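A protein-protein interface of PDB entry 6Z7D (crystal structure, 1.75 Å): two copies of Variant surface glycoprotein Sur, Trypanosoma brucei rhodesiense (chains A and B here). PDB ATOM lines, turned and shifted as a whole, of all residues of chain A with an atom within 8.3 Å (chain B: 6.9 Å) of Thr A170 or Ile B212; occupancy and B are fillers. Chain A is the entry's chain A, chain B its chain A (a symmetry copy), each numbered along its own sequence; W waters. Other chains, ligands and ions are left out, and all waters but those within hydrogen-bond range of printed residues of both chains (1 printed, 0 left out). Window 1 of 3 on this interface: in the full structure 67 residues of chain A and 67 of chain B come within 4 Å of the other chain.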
ATOM      1  N   ALA A 134     -23.738 -16.597   0.205  1.00  0.00           N
ATOM      2  CA  ALA A 134     -24.258 -17.890   0.620  1.00  0.00           C
ATOM      3  C   ALA A 134     -23.176 -18.948   0.516  1.00  0.00           C
ATOM      4  O   ALA A 134     -23.112 -19.865   1.350  1.00  0.00           O
ATOM      5  CB  ALA A 134     -25.466 -18.270  -0.249  1.00  0.00           C
ATOM      6  N   GLN A 136     -19.971 -18.654   0.953  1.00  0.00           N
ATOM      7  CA  GLN A 136     -19.072 -18.596   2.109  1.00  0.00           C
ATOM      8  C   GLN A 136     -19.676 -19.282   3.339  1.00  0.00           C
ATOM      9  O   GLN A 136     -18.996 -20.035   4.054  1.00  0.00           O
ATOM     10  CB  GLN A 136     -18.732 -17.118   2.369  1.00  0.00           C
ATOM     11  CG  GLN A 136     -17.843 -16.894   3.623  1.00  0.00           C
ATOM     12  CD  GLN A 136     -16.431 -17.493   3.404  1.00  0.00           C
ATOM     13  OE1 GLN A 136     -15.763 -17.199   2.394  1.00  0.00           O
ATOM     14  NE2 GLN A 136     -15.957 -18.296   4.370  1.00  0.00           N
ATOM     15  N   ILE A 137     -20.958 -19.066   3.594  1.00  0.00           N
ATOM     16  CA  ILE A 137     -21.633 -19.708   4.727  1.00  0.00           C
ATOM     17  C   ILE A 137     -21.799 -21.217   4.496  1.00  0.00           C
ATOM     18  O   ILE A 137     -21.578 -22.027   5.420  1.00  0.00           O
ATOM     19  CB  ILE A 137     -22.965 -18.985   4.979  1.00  0.00           C
ATOM     20  CG1 ILE A 137     -22.601 -17.563   5.443  1.00  0.00           C
ATOM     21  CG2 ILE A 137     -23.801 -19.789   6.026  1.00  0.00           C
ATOM     22  CD1 ILE A 137     -23.805 -16.547   5.562  1.00  0.00           C
ATOM     23  N   GLN A 138     -22.136 -21.632   3.263  1.00  0.00           N
ATOM     24  CA  GLN A 138     -22.362 -23.054   3.012  1.00  0.00           C
ATOM     25  C   GLN A 138     -21.064 -23.829   3.014  1.00  0.00           C
ATOM     26  O   GLN A 138     -21.108 -25.066   3.136  1.00  0.00           O
ATOM     27  CB  GLN A 138     -23.123 -23.307   1.684  1.00  0.00           C
ATOM     28  CG  GLN A 138     -24.574 -22.692   1.664  1.00  0.00           C
ATOM     29  CD  GLN A 138     -25.511 -23.335   2.698  1.00  0.00           C
ATOM     30  OE1 GLN A 138     -25.166 -24.337   3.390  1.00  0.00           O
ATOM     31  NE2 GLN A 138     -26.682 -22.762   2.827  1.00  0.00           N
ATOM     32  N   ALA A 139     -19.927 -23.128   2.986  1.00  0.00           N
ATOM     33  CA  ALA A 139     -18.619 -23.771   3.123  1.00  0.00           C
ATOM     34  C   ALA A 139     -18.259 -24.081   4.576  1.00  0.00           C
ATOM     35  O   ALA A 139     -17.241 -24.770   4.825  1.00  0.00           O
ATOM     36  CB  ALA A 139     -17.516 -22.856   2.530  1.00  0.00           C
ATOM     37  N   ALA A 140     -19.041 -23.581   5.550  1.00  0.00           N
ATOM     38  CA  ALA A 140     -18.726 -23.773   6.972  1.00  0.00           C
ATOM     39  C   ALA A 140     -19.265 -25.129   7.357  1.00  0.00           C
ATOM     40  O   ALA A 140     -20.423 -25.281   7.806  1.00  0.00           O
ATOM     41  CB  ALA A 140     -19.347 -22.687   7.846  1.00  0.00           C
ATOM     42  N   GLN A 141     -18.432 -26.147   7.128  1.00  0.00           N
ATOM     43  CA  GLN A 141     -18.889 -27.521   7.123  1.00  0.00           C
ATOM     44  C   GLN A 141     -18.345 -28.341   8.277  1.00  0.00           C
ATOM     45  O   GLN A 141     -18.739 -29.521   8.419  1.00  0.00           O
ATOM     46  CB  GLN A 141     -18.502 -28.173   5.779  1.00  0.00           C
ATOM     47  CG  GLN A 141     -19.324 -27.508   4.699  1.00  0.00           C
ATOM     48  CD  GLN A 141     -19.295 -28.252   3.389  1.00  0.00           C
ATOM     49  OE1 GLN A 141     -18.649 -29.272   3.259  1.00  0.00           O
ATOM     50  NE2 GLN A 141     -20.026 -27.751   2.423  1.00  0.00           N
ATOM     51  N   GLN A 142     -17.477 -27.762   9.118  1.00  0.00           N
ATOM     52  CA  GLN A 142     -16.982 -28.464  10.290  1.00  0.00           C
ATOM     53  C   GLN A 142     -17.302 -27.647  11.526  1.00  0.00           C
ATOM     54  O   GLN A 142     -16.997 -26.454  11.573  1.00  0.00           O
ATOM     55  CB  GLN A 142     -15.466 -28.708  10.223  1.00  0.00           C
ATOM     56  CG  GLN A 142     -15.024 -29.387   8.928  1.00  0.00           C
ATOM     57  CD  GLN A 142     -13.520 -29.389   8.752  1.00  0.00           C
ATOM     58  OE1 GLN A 142     -12.772 -29.880   9.611  1.00  0.00           O
ATOM     59  NE2 GLN A 142     -13.066 -28.823   7.654  1.00  0.00           N
ATOM     60  N   ALA A 143     -17.844 -28.313  12.538  1.00  0.00           N
ATOM     61  CA  ALA A 143     -18.250 -27.654  13.772  1.00  0.00           C
ATOM     62  C   ALA A 143     -17.097 -27.659  14.764  1.00  0.00           C
ATOM     63  O   ALA A 143     -16.318 -28.612  14.805  1.00  0.00           O
ATOM     64  CB  ALA A 143     -19.435 -28.398  14.409  1.00  0.00           C
ATOM     65  N   THR A 144     -17.021 -26.608  15.590  1.00  0.00           N
ATOM     66  CA  THR A 144     -16.160 -26.572  16.773  1.00  0.00           C
ATOM     67  C   THR A 144     -17.064 -26.724  17.963  1.00  0.00           C
ATOM     68  O   THR A 144     -17.883 -25.829  18.207  1.00  0.00           O
ATOM     69  CB  THR A 144     -15.416 -25.237  16.901  1.00  0.00           C
ATOM     70  OG1 THR A 144     -14.642 -25.006  15.731  1.00  0.00           O
ATOM     71  CG2 THR A 144     -14.542 -25.199  18.182  1.00  0.00           C
ATOM     72  N   LEU A 145     -16.889 -27.812  18.724  1.00  0.00           N
ATOM     73  CA  LEU A 145     -17.685 -28.018  19.926  1.00  0.00           C
ATOM     74  C   LEU A 145     -17.216 -27.137  21.073  1.00  0.00           C
ATOM     75  O   LEU A 145     -16.018 -26.890  21.250  1.00  0.00           O
ATOM     76  CB  LEU A 145     -17.629 -29.466  20.390  1.00  0.00           C
ATOM     77  CG  LEU A 145     -18.443 -30.484  19.616  1.00  0.00           C
ATOM     78  CD1 LEU A 145     -18.318 -31.844  20.374  1.00  0.00           C
ATOM     79  CD2 LEU A 145     -19.904 -30.017  19.465  1.00  0.00           C
ATOM     80  N   THR A 146     -18.168 -26.695  21.876  1.00  0.00           N
ATOM     81  CA  THR A 146     -17.814 -26.072  23.130  1.00  0.00           C
ATOM     82  C   THR A 146     -17.823 -27.112  24.243  1.00  0.00           C
ATOM     83  O   THR A 146     -18.280 -28.253  24.072  1.00  0.00           O
ATOM     84  CB  THR A 146     -18.787 -24.936  23.452  1.00  0.00           C
ATOM     85  OG1 THR A 146     -20.118 -25.406  23.243  1.00  0.00           O
ATOM     86  CG2 THR A 146     -18.545 -23.788  22.532  1.00  0.00           C
ATOM     87  N   GLU A 167     -23.673 -25.017  24.420  1.00  0.00           N
ATOM     88  CA  GLU A 167     -24.051 -23.701  23.928  1.00  0.00           C
ATOM     89  C   GLU A 167     -22.960 -23.163  23.019  1.00  0.00           C
ATOM     90  O   GLU A 167     -21.771 -23.321  23.313  1.00  0.00           O
ATOM     91  CB  GLU A 167     -24.286 -22.718  25.096  1.00  0.00           C
ATOM     92  CG  GLU A 167     -25.449 -23.177  25.990  1.00  0.00           C
ATOM     93  CD  GLU A 167     -25.640 -22.351  27.266  1.00  0.00           C
ATOM     94  OE1 GLU A 167     -25.085 -21.242  27.385  1.00  0.00           O
ATOM     95  OE2 GLU A 167     -26.357 -22.838  28.162  1.00  0.00           O
ATOM     96  N   GLY A 168     -23.370 -22.525  21.921  1.00  0.00           N
ATOM     97  CA  GLY A 168     -22.407 -21.815  21.082  1.00  0.00           C
ATOM     98  C   GLY A 168     -21.478 -22.706  20.272  1.00  0.00           C
ATOM     99  O   GLY A 168     -20.328 -22.327  20.010  1.00  0.00           O
ATOM    100  N   ILE A 169     -21.948 -23.875  19.849  1.00  0.00           N
ATOM    101  CA  ILE A 169     -21.237 -24.597  18.796  1.00  0.00           C
ATOM    102  C   ILE A 169     -21.160 -23.703  17.566  1.00  0.00           C
ATOM    103  O   ILE A 169     -22.140 -23.066  17.206  1.00  0.00           O
ATOM    104  CB  ILE A 169     -21.955 -25.913  18.470  1.00  0.00           C
ATOM    105  CG1 ILE A 169     -21.892 -26.833  19.696  1.00  0.00           C
ATOM    106  CG2 ILE A 169     -21.314 -26.576  17.215  1.00  0.00           C
ATOM    107  CD1 ILE A 169     -22.900 -28.027  19.653  1.00  0.00           C
ATOM    108  N   THR A 170     -19.993 -23.649  16.890  1.00  0.00           N
ATOM    109  CA  THR A 170     -19.948 -22.815  15.702  1.00  0.00           C
ATOM    110  C   THR A 170     -19.331 -23.595  14.547  1.00  0.00           C
ATOM    111  O   THR A 170     -18.585 -24.582  14.745  1.00  0.00           O
ATOM    112  CB  THR A 170     -19.122 -21.521  15.917  1.00  0.00           C
ATOM    113  OG1 THR A 170     -17.823 -21.887  16.381  1.00  0.00           O
ATOM    114  CG2 THR A 170     -19.803 -20.555  16.999  1.00  0.00           C
ATOM    115  N   ALA A 171     -19.592 -23.083  13.347  1.00  0.00           N
ATOM    116  CA  ALA A 171     -18.926 -23.556  12.130  1.00  0.00           C
ATOM    117  C   ALA A 171     -18.523 -22.330  11.325  1.00  0.00           C
ATOM    118  O   ALA A 171     -19.370 -21.449  11.071  1.00  0.00           O
ATOM    119  CB  ALA A 171     -19.847 -24.460  11.272  1.00  0.00           C
ATOM    120  N   THR A 172     -17.250 -22.276  10.890  1.00  0.00           N
ATOM    121  CA  THR A 172     -16.739 -21.171  10.074  1.00  0.00           C
ATOM    122  C   THR A 172     -15.778 -21.740   9.031  1.00  0.00           C
ATOM    123  O   THR A 172     -14.964 -22.600   9.365  1.00  0.00           O
ATOM    124  CB  THR A 172     -15.938 -20.157  10.930  1.00  0.00           C
ATOM    125  OG1 THR A 172     -16.702 -19.814  12.102  1.00  0.00           O
ATOM    126  CG2 THR A 172     -15.673 -18.885  10.095  1.00  0.00           C
ATOM    127  N   ALA A 173     -15.810 -21.248   7.807  1.00  0.00           N
ATOM    128  CA  ALA A 173     -14.812 -21.683   6.833  1.00  0.00           C
ATOM    129  C   ALA A 173     -13.784 -20.590   6.663  1.00  0.00           C
ATOM    130  O   ALA A 173     -14.079 -19.416   6.876  1.00  0.00           O
ATOM    131  CB  ALA A 173     -15.466 -21.957   5.481  1.00  0.00           C
ATOM    132  N   THR A 211     -31.144 -22.168   3.683  1.00  0.00           N
ATOM    133  CA  THR A 211     -31.257 -23.313   4.573  1.00  0.00           C
ATOM    134  C   THR A 211     -29.900 -23.720   5.099  1.00  0.00           C
ATOM    135  O   THR A 211     -28.965 -23.923   4.311  1.00  0.00           O
ATOM    136  CB  THR A 211     -31.934 -24.474   3.825  1.00  0.00           C
ATOM    137  OG1 THR A 211     -33.257 -24.032   3.546  1.00  0.00           O
ATOM    138  CG2 THR A 211     -31.993 -25.747   4.662  1.00  0.00           C
ATOM    139  N   ILE A 212     -29.834 -23.945   6.425  1.00  0.00           N
ATOM    140  CA  ILE A 212     -28.681 -24.593   7.061  1.00  0.00           C
ATOM    141  C   ILE A 212     -28.993 -26.074   7.191  1.00  0.00           C
ATOM    142  O   ILE A 212     -30.109 -26.431   7.565  1.00  0.00           O
ATOM    143  CB  ILE A 212     -28.408 -23.975   8.447  1.00  0.00           C
ATOM    144  CG1 ILE A 212     -28.068 -22.497   8.306  1.00  0.00           C
ATOM    145  CG2 ILE A 212     -27.283 -24.799   9.196  1.00  0.00           C
ATOM    146  CD1 ILE A 212     -28.120 -21.761   9.609  1.00  0.00           C
ATOM    147  N   THR A 213     -28.036 -26.942   6.855  1.00  0.00           N
ATOM    148  CA  THR A 213     -28.198 -28.401   6.934  1.00  0.00           C
ATOM    149  C   THR A 213     -27.070 -28.967   7.770  1.00  0.00           C
ATOM    150  O   THR A 213     -25.915 -28.524   7.637  1.00  0.00           O
ATOM    151  CB  THR A 213     -28.162 -29.071   5.514  1.00  0.00           C
ATOM    152  OG1 THR A 213     -29.151 -28.432   4.674  1.00  0.00           O
ATOM    153  CG2 THR A 213     -28.568 -30.584   5.624  1.00  0.00           C
ATOM    154  N   LEU A 214     -27.375 -29.982   8.586  1.00  0.00           N
ATOM    155  CA  LEU A 214     -26.306 -30.581   9.366  1.00  0.00           C
ATOM    156  C   LEU A 214     -26.701 -32.007   9.754  1.00  0.00           C
ATOM    157  O   LEU A 214     -27.879 -32.407   9.704  1.00  0.00           O
ATOM    158  CB  LEU A 214     -26.004 -29.711  10.586  1.00  0.00           C
ATOM    159  CG  LEU A 214     -27.167 -29.645  11.618  1.00  0.00           C
ATOM    160  CD1 LEU A 214     -26.983 -30.711  12.738  1.00  0.00           C
ATOM    161  CD2 LEU A 214     -27.361 -28.273  12.243  1.00  0.00           C
ATOM    162  N   VAL A 256     -21.735 -32.591  16.113  1.00  0.00           N
ATOM    163  CA  VAL A 256     -22.240 -32.182  14.815  1.00  0.00           C
ATOM    164  C   VAL A 256     -21.171 -32.624  13.820  1.00  0.00           C
ATOM    165  O   VAL A 256     -20.070 -32.067  13.814  1.00  0.00           O
ATOM    166  CB  VAL A 256     -22.473 -30.670  14.759  1.00  0.00           C
ATOM    167  CG1 VAL A 256     -22.901 -30.263  13.391  1.00  0.00           C
ATOM    168  CG2 VAL A 256     -23.524 -30.257  15.817  1.00  0.00           C
ATOM    169  N   LEU A 259     -21.789 -29.982   8.313  1.00  0.00           N
ATOM    170  CA  LEU A 259     -22.821 -29.021   7.922  1.00  0.00           C
ATOM    171  C   LEU A 259     -22.650 -28.756   6.437  1.00  0.00           C
ATOM    172  O   LEU A 259     -21.636 -29.146   5.836  1.00  0.00           O
ATOM    173  CB  LEU A 259     -22.729 -27.676   8.688  1.00  0.00           C
ATOM    174  CG  LEU A 259     -22.652 -27.756  10.238  1.00  0.00           C
ATOM    175  CD1 LEU A 259     -21.234 -27.910  10.762  1.00  0.00           C
ATOM    176  CD2 LEU A 259     -23.328 -26.519  10.878  1.00  0.00           C
ATOM    177  N   GLY A 260     -23.664 -28.111   5.865  1.00  0.00           N
ATOM    178  CA  GLY A 260     -23.592 -27.585   4.500  1.00  0.00           C
ATOM    179  C   GLY A 260     -24.761 -28.093   3.681  1.00  0.00           C
ATOM    180  O   GLY A 260     -25.061 -29.292   3.678  1.00  0.00           O
ATOM    181  N   THR A 261     -25.400 -27.192   2.947  1.00  0.00           N
ATOM    182  CA  THR A 261     -26.533 -27.526   2.086  1.00  0.00           C
ATOM    183  C   THR A 261     -26.012 -27.719   0.669  1.00  0.00           C
ATOM    184  O   THR A 261     -25.192 -26.923   0.204  1.00  0.00           O
ATOM    185  CB  THR A 261     -27.542 -26.385   2.144  1.00  0.00           C
ATOM    186  OG1 THR A 261     -27.949 -26.216   3.527  1.00  0.00           O
ATOM    187  CG2 THR A 261     -28.771 -26.648   1.186  1.00  0.00           C
ATOM    188  N   ILE B 137     -30.049 -16.080   6.123  1.00  0.00           N
ATOM    189  CA  ILE B 137     -29.515 -17.316   6.703  1.00  0.00           C
ATOM    190  C   ILE B 137     -29.456 -17.235   8.235  1.00  0.00           C
ATOM    191  O   ILE B 137     -29.810 -18.207   8.934  1.00  0.00           O
ATOM    192  CB  ILE B 137     -28.151 -17.611   6.060  1.00  0.00           C
ATOM    193  CG1 ILE B 137     -28.430 -17.915   4.577  1.00  0.00           C
ATOM    194  CG2 ILE B 137     -27.464 -18.790   6.821  1.00  0.00           C
ATOM    195  CD1 ILE B 137     -27.160 -18.041   3.647  1.00  0.00           C
ATOM    196  N   GLN B 138     -29.063 -16.076   8.790  1.00  0.00           N
ATOM    197  CA  GLN B 138     -28.936 -15.972  10.242  1.00  0.00           C
ATOM    198  C   GLN B 138     -30.289 -15.937  10.914  1.00  0.00           C
ATOM    199  O   GLN B 138     -30.355 -16.172  12.134  1.00  0.00           O
ATOM    200  CB  GLN B 138     -28.101 -14.738  10.676  1.00  0.00           C
ATOM    201  CG  GLN B 138     -26.607 -14.782  10.175  1.00  0.00           C
ATOM    202  CD  GLN B 138     -25.805 -15.942  10.785  1.00  0.00           C
ATOM    203  OE1 GLN B 138     -26.282 -16.690  11.689  1.00  0.00           O
ATOM    204  NE2 GLN B 138     -24.604 -16.115  10.291  1.00  0.00           N
ATOM    205  N   LYS B 207     -18.195 -12.081  11.551  1.00  0.00           N
ATOM    206  CA  LYS B 207     -18.759 -13.365  11.986  1.00  0.00           C
ATOM    207  C   LYS B 207     -20.191 -13.556  11.485  1.00  0.00           C
ATOM    208  O   LYS B 207     -20.617 -14.693  11.222  1.00  0.00           O
ATOM    209  CB  LYS B 207     -18.712 -13.411  13.516  1.00  0.00           C
ATOM    210  CG  LYS B 207     -19.020 -14.671  14.214  1.00  0.00           C
ATOM    211  CD  LYS B 207     -19.092 -14.423  15.770  1.00  0.00           C
ATOM    212  CE  LYS B 207     -19.978 -13.189  16.174  1.00  0.00           C
ATOM    213  NZ  LYS B 207     -20.461 -13.037  17.629  1.00  0.00           N
ATOM    214  N   TYR B 208     -20.952 -12.466  11.366  1.00  0.00           N
ATOM    215  CA  TYR B 208     -22.348 -12.565  10.916  1.00  0.00           C
ATOM    216  C   TYR B 208     -22.425 -13.099   9.501  1.00  0.00           C
ATOM    217  O   TYR B 208     -23.432 -13.743   9.122  1.00  0.00           O
ATOM    218  CB  TYR B 208     -22.999 -11.183  11.010  1.00  0.00           C
ATOM    219  CG  TYR B 208     -24.489 -11.173  10.933  1.00  0.00           C
ATOM    220  CD1 TYR B 208     -25.287 -11.593  12.030  1.00  0.00           C
ATOM    221  CD2 TYR B 208     -25.110 -10.708   9.770  1.00  0.00           C
ATOM    222  CE1 TYR B 208     -26.700 -11.536  11.933  1.00  0.00           C
ATOM    223  CE2 TYR B 208     -26.505 -10.665   9.642  1.00  0.00           C
ATOM    224  CZ  TYR B 208     -27.276 -11.057  10.749  1.00  0.00           C
ATOM    225  OH  TYR B 208     -28.632 -11.020  10.613  1.00  0.00           O
ATOM    226  N   THR B 210     -19.950 -15.119   8.164  1.00  0.00           N
ATOM    227  CA  THR B 210     -19.140 -16.316   7.945  1.00  0.00           C
ATOM    228  C   THR B 210     -19.456 -17.483   8.861  1.00  0.00           C
ATOM    229  O   THR B 210     -19.003 -18.587   8.569  1.00  0.00           O
ATOM    230  CB  THR B 210     -17.659 -16.010   8.147  1.00  0.00           C
ATOM    231  OG1 THR B 210     -17.517 -15.654   9.519  1.00  0.00           O
ATOM    232  CG2 THR B 210     -17.211 -14.803   7.304  1.00  0.00           C
ATOM    233  N   THR B 211     -20.185 -17.276   9.952  1.00  0.00           N
ATOM    234  CA  THR B 211     -20.232 -18.271  11.012  1.00  0.00           C
ATOM    235  C   THR B 211     -21.653 -18.718  11.265  1.00  0.00           C
ATOM    236  O   THR B 211     -22.541 -17.878  11.472  1.00  0.00           O
ATOM    237  CB  THR B 211     -19.599 -17.687  12.286  1.00  0.00           C
ATOM    238  OG1 THR B 211     -18.227 -17.478  11.972  1.00  0.00           O
ATOM    239  CG2 THR B 211     -19.706 -18.636  13.475  1.00  0.00           C
ATOM    240  N   ILE B 212     -21.836 -20.049  11.357  1.00  0.00           N
ATOM    241  CA  ILE B 212     -23.082 -20.644  11.854  1.00  0.00           C
ATOM    242  C   ILE B 212     -22.902 -20.931  13.335  1.00  0.00           C
ATOM    243  O   ILE B 212     -21.850 -21.426  13.737  1.00  0.00           O
ATOM    244  CB  ILE B 212     -23.406 -21.943  11.088  1.00  0.00           C
ATOM    245  CG1 ILE B 212     -23.613 -21.643   9.609  1.00  0.00           C
ATOM    246  CG2 ILE B 212     -24.647 -22.668  11.751  1.00  0.00           C
ATOM    247  CD1 ILE B 212     -23.598 -22.875   8.758  1.00  0.00           C
ATOM    248  N   THR B 213     -23.900 -20.597  14.158  1.00  0.00           N
ATOM    249  CA  THR B 213     -23.863 -20.818  15.610  1.00  0.00           C
ATOM    250  C   THR B 213     -25.093 -21.607  16.009  1.00  0.00           C
ATOM    251  O   THR B 213     -26.195 -21.341  15.496  1.00  0.00           O
ATOM    252  CB  THR B 213     -23.848 -19.466  16.408  1.00  0.00           C
ATOM    253  OG1 THR B 213     -22.751 -18.656  15.927  1.00  0.00           O
ATOM    254  CG2 THR B 213     -23.577 -19.743  17.930  1.00  0.00           C
ATOM    255  N   LEU B 214     -24.933 -22.533  16.961  1.00  0.00           N
ATOM    256  CA  LEU B 214     -26.102 -23.272  17.402  1.00  0.00           C
ATOM    257  C   LEU B 214     -25.856 -23.817  18.809  1.00  0.00           C
ATOM    258  O   LEU B 214     -24.713 -23.900  19.299  1.00  0.00           O
ATOM    259  CB  LEU B 214     -26.422 -24.382  16.399  1.00  0.00           C
ATOM    260  CG  LEU B 214     -25.338 -25.495  16.322  1.00  0.00           C
ATOM    261  CD1 LEU B 214     -25.691 -26.687  17.259  1.00  0.00           C
ATOM    262  CD2 LEU B 214     -25.079 -26.009  14.915  1.00  0.00           C
ATOM    263  N   LEU B 259     -30.465 -21.805  16.571  1.00  0.00           N
ATOM    264  CA  LEU B 259     -29.331 -21.416  15.732  1.00  0.00           C
ATOM    265  C   LEU B 259     -29.369 -19.905  15.598  1.00  0.00           C
ATOM    266  O   LEU B 259     -30.364 -19.260  15.966  1.00  0.00           O
ATOM    267  CB  LEU B 259     -29.371 -22.049  14.317  1.00  0.00           C
ATOM    268  CG  LEU B 259     -29.568 -23.588  14.243  1.00  0.00           C
ATOM    269  CD1 LEU B 259     -31.029 -24.007  14.240  1.00  0.00           C
ATOM    270  CD2 LEU B 259     -28.844 -24.169  13.004  1.00  0.00           C
ATOM    271  N   GLY B 260     -28.267 -19.362  15.087  1.00  0.00           N
ATOM    272  CA  GLY B 260     -28.193 -17.953  14.689  1.00  0.00           C
ATOM    273  C   GLY B 260     -27.013 -17.281  15.358  1.00  0.00           C
ATOM    274  O   GLY B 260     -26.812 -17.410  16.572  1.00  0.00           O
ATOM    275  N   THR B 261     -26.249 -16.524  14.582  1.00  0.00           N
ATOM    276  CA  THR B 261     -25.086 -15.792  15.080  1.00  0.00           C
ATOM    277  C   THR B 261     -25.514 -14.360  15.368  1.00  0.00           C
ATOM    278  O   THR B 261     -26.230 -13.761  14.560  1.00  0.00           O
ATOM    279  CB  THR B 261     -23.995 -15.831  14.017  1.00  0.00           C
ATOM    280  OG1 THR B 261     -23.679 -17.222  13.747  1.00  0.00           O
ATOM    281  CG2 THR B 261     -22.723 -15.004  14.461  1.00  0.00           C
HETATM  282  O   HOH W   1     -17.750 -19.404   6.450  1.00  0.00           O
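Water W1 lies within hydrogen-bond range of the backbone carbonyl oxygen of Thr B210, the backbone carbonyl oxygen of Gln A136 and the backbone NH of Ala A173.
N of Gly A168 sits at hydrogen-bond distance from O of Leu B214 (3.3 Å). N of Ile A169 sits at hydrogen-bond distance from O of Leu B214, at 2.8 Å. The backbone NH (N) of Ala A171 is in hydrogen-bond range of the backbone carbonyl oxygen (O) of Ile B212 (2.8 Å). OG1 of Thr A172 sits at hydrogen-bond distance from OG1 of Thr B211, at 2.8 Å.
The backbone NH of Thr A144 is in hydrogen-bond range of the backbone carbonyl oxygen of Thr A170, 2.7 Å away. The side-chain amide nitrogen of Gln B138 is in hydrogen-bond range of the backbone carbonyl oxygen of Thr B211, 3.0 Å away. The side-chain hydroxyl (OG1) of Thr B211 is in hydrogen-bond range of the side-chain hydroxyl (OG1) of Thr B210 (3.1 Å). The backbone carbonyl oxygen (O) of Thr B211 is in hydrogen-bond range of the side-chain hydroxyl (OG1) of Thr B261. The backbone carbonyl oxygen of Thr B213 sits at hydrogen-bond distance from the backbone NH of Gly B260, at 2.9 Å. OG1 of Thr B213 sits at hydrogen-bond distance from OG1 of Thr B261.
Thr A170 touches three residues of chain B. Of the printed residues of chain A, Ile B212 touches Ile A137, Ile A169, Thr A170 and Ala A171. Thr B213 touches just these residues of chain A: Gly A168, Ile A169 and Thr A170. Printed residues of chain A within 4 Å of Thr B210: Ala A171 (3.8 Å) and Thr A172 (3.7 Å). Of the printed residues of chain B, Ile A137 touches Ile B137 (3.9 Å) and Ile B212 (3.99 Å). Printed residues of chain A within 4 Å of Thr B211: Thr A170, Ala A171 and Thr A172. Printed residues of chain A within 4 Å of Leu B214: Gly A168 (3.3 Å) and Ile A169 (2.8 Å). Of the printed residues of chain A, Ile B137 touches Ile A137 and Ile A212. The nearest printed residue of chain A that does not touch Ile B212 is Ala A140 (4.1 Å).
Hydrophobic or aromatic side chains of chain B that line the printed part of chain A: Ile B137, Ile B212 and Leu B214. Hydrophobic or aromatic side chains of chain A within 4 Å of the printed part of chain B: Ile A137, Ile A169 and Ile A212.
Ile A137 touches its own counterpart, Ile B137. Ile A137 touches Ile B212, and with the chains exchanged Ile A212 touches Ile B137. Of the 16 pairs that touch across the chains among the printed residues, 3 have their exchanged pair printed and touching as well.
Among the printed residues, pairs that only touch across the chains: Thr A170 with Ile B212 (3.1 Å), Ile A169 with Thr B213 (3.3 Å), Ala A171 with Thr B211 (3.3 Å), Thr A170 with Thr B213 (3.7 Å), Thr A172 with Thr B210 (3.7 Å), Ala A171 with Thr B210 (3.8 Å), Thr A170 with Thr B211 (3.8 Å), Ile A169 with Ile B212 (3.8 Å), Ile A137 with Ile B137 (3.9 Å), Gly A168 with Thr B213 (3.9 Å), Ile A137 with Ile B212 (3.99 Å) and Ile A212 with Ile B137 (3.99 Å).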
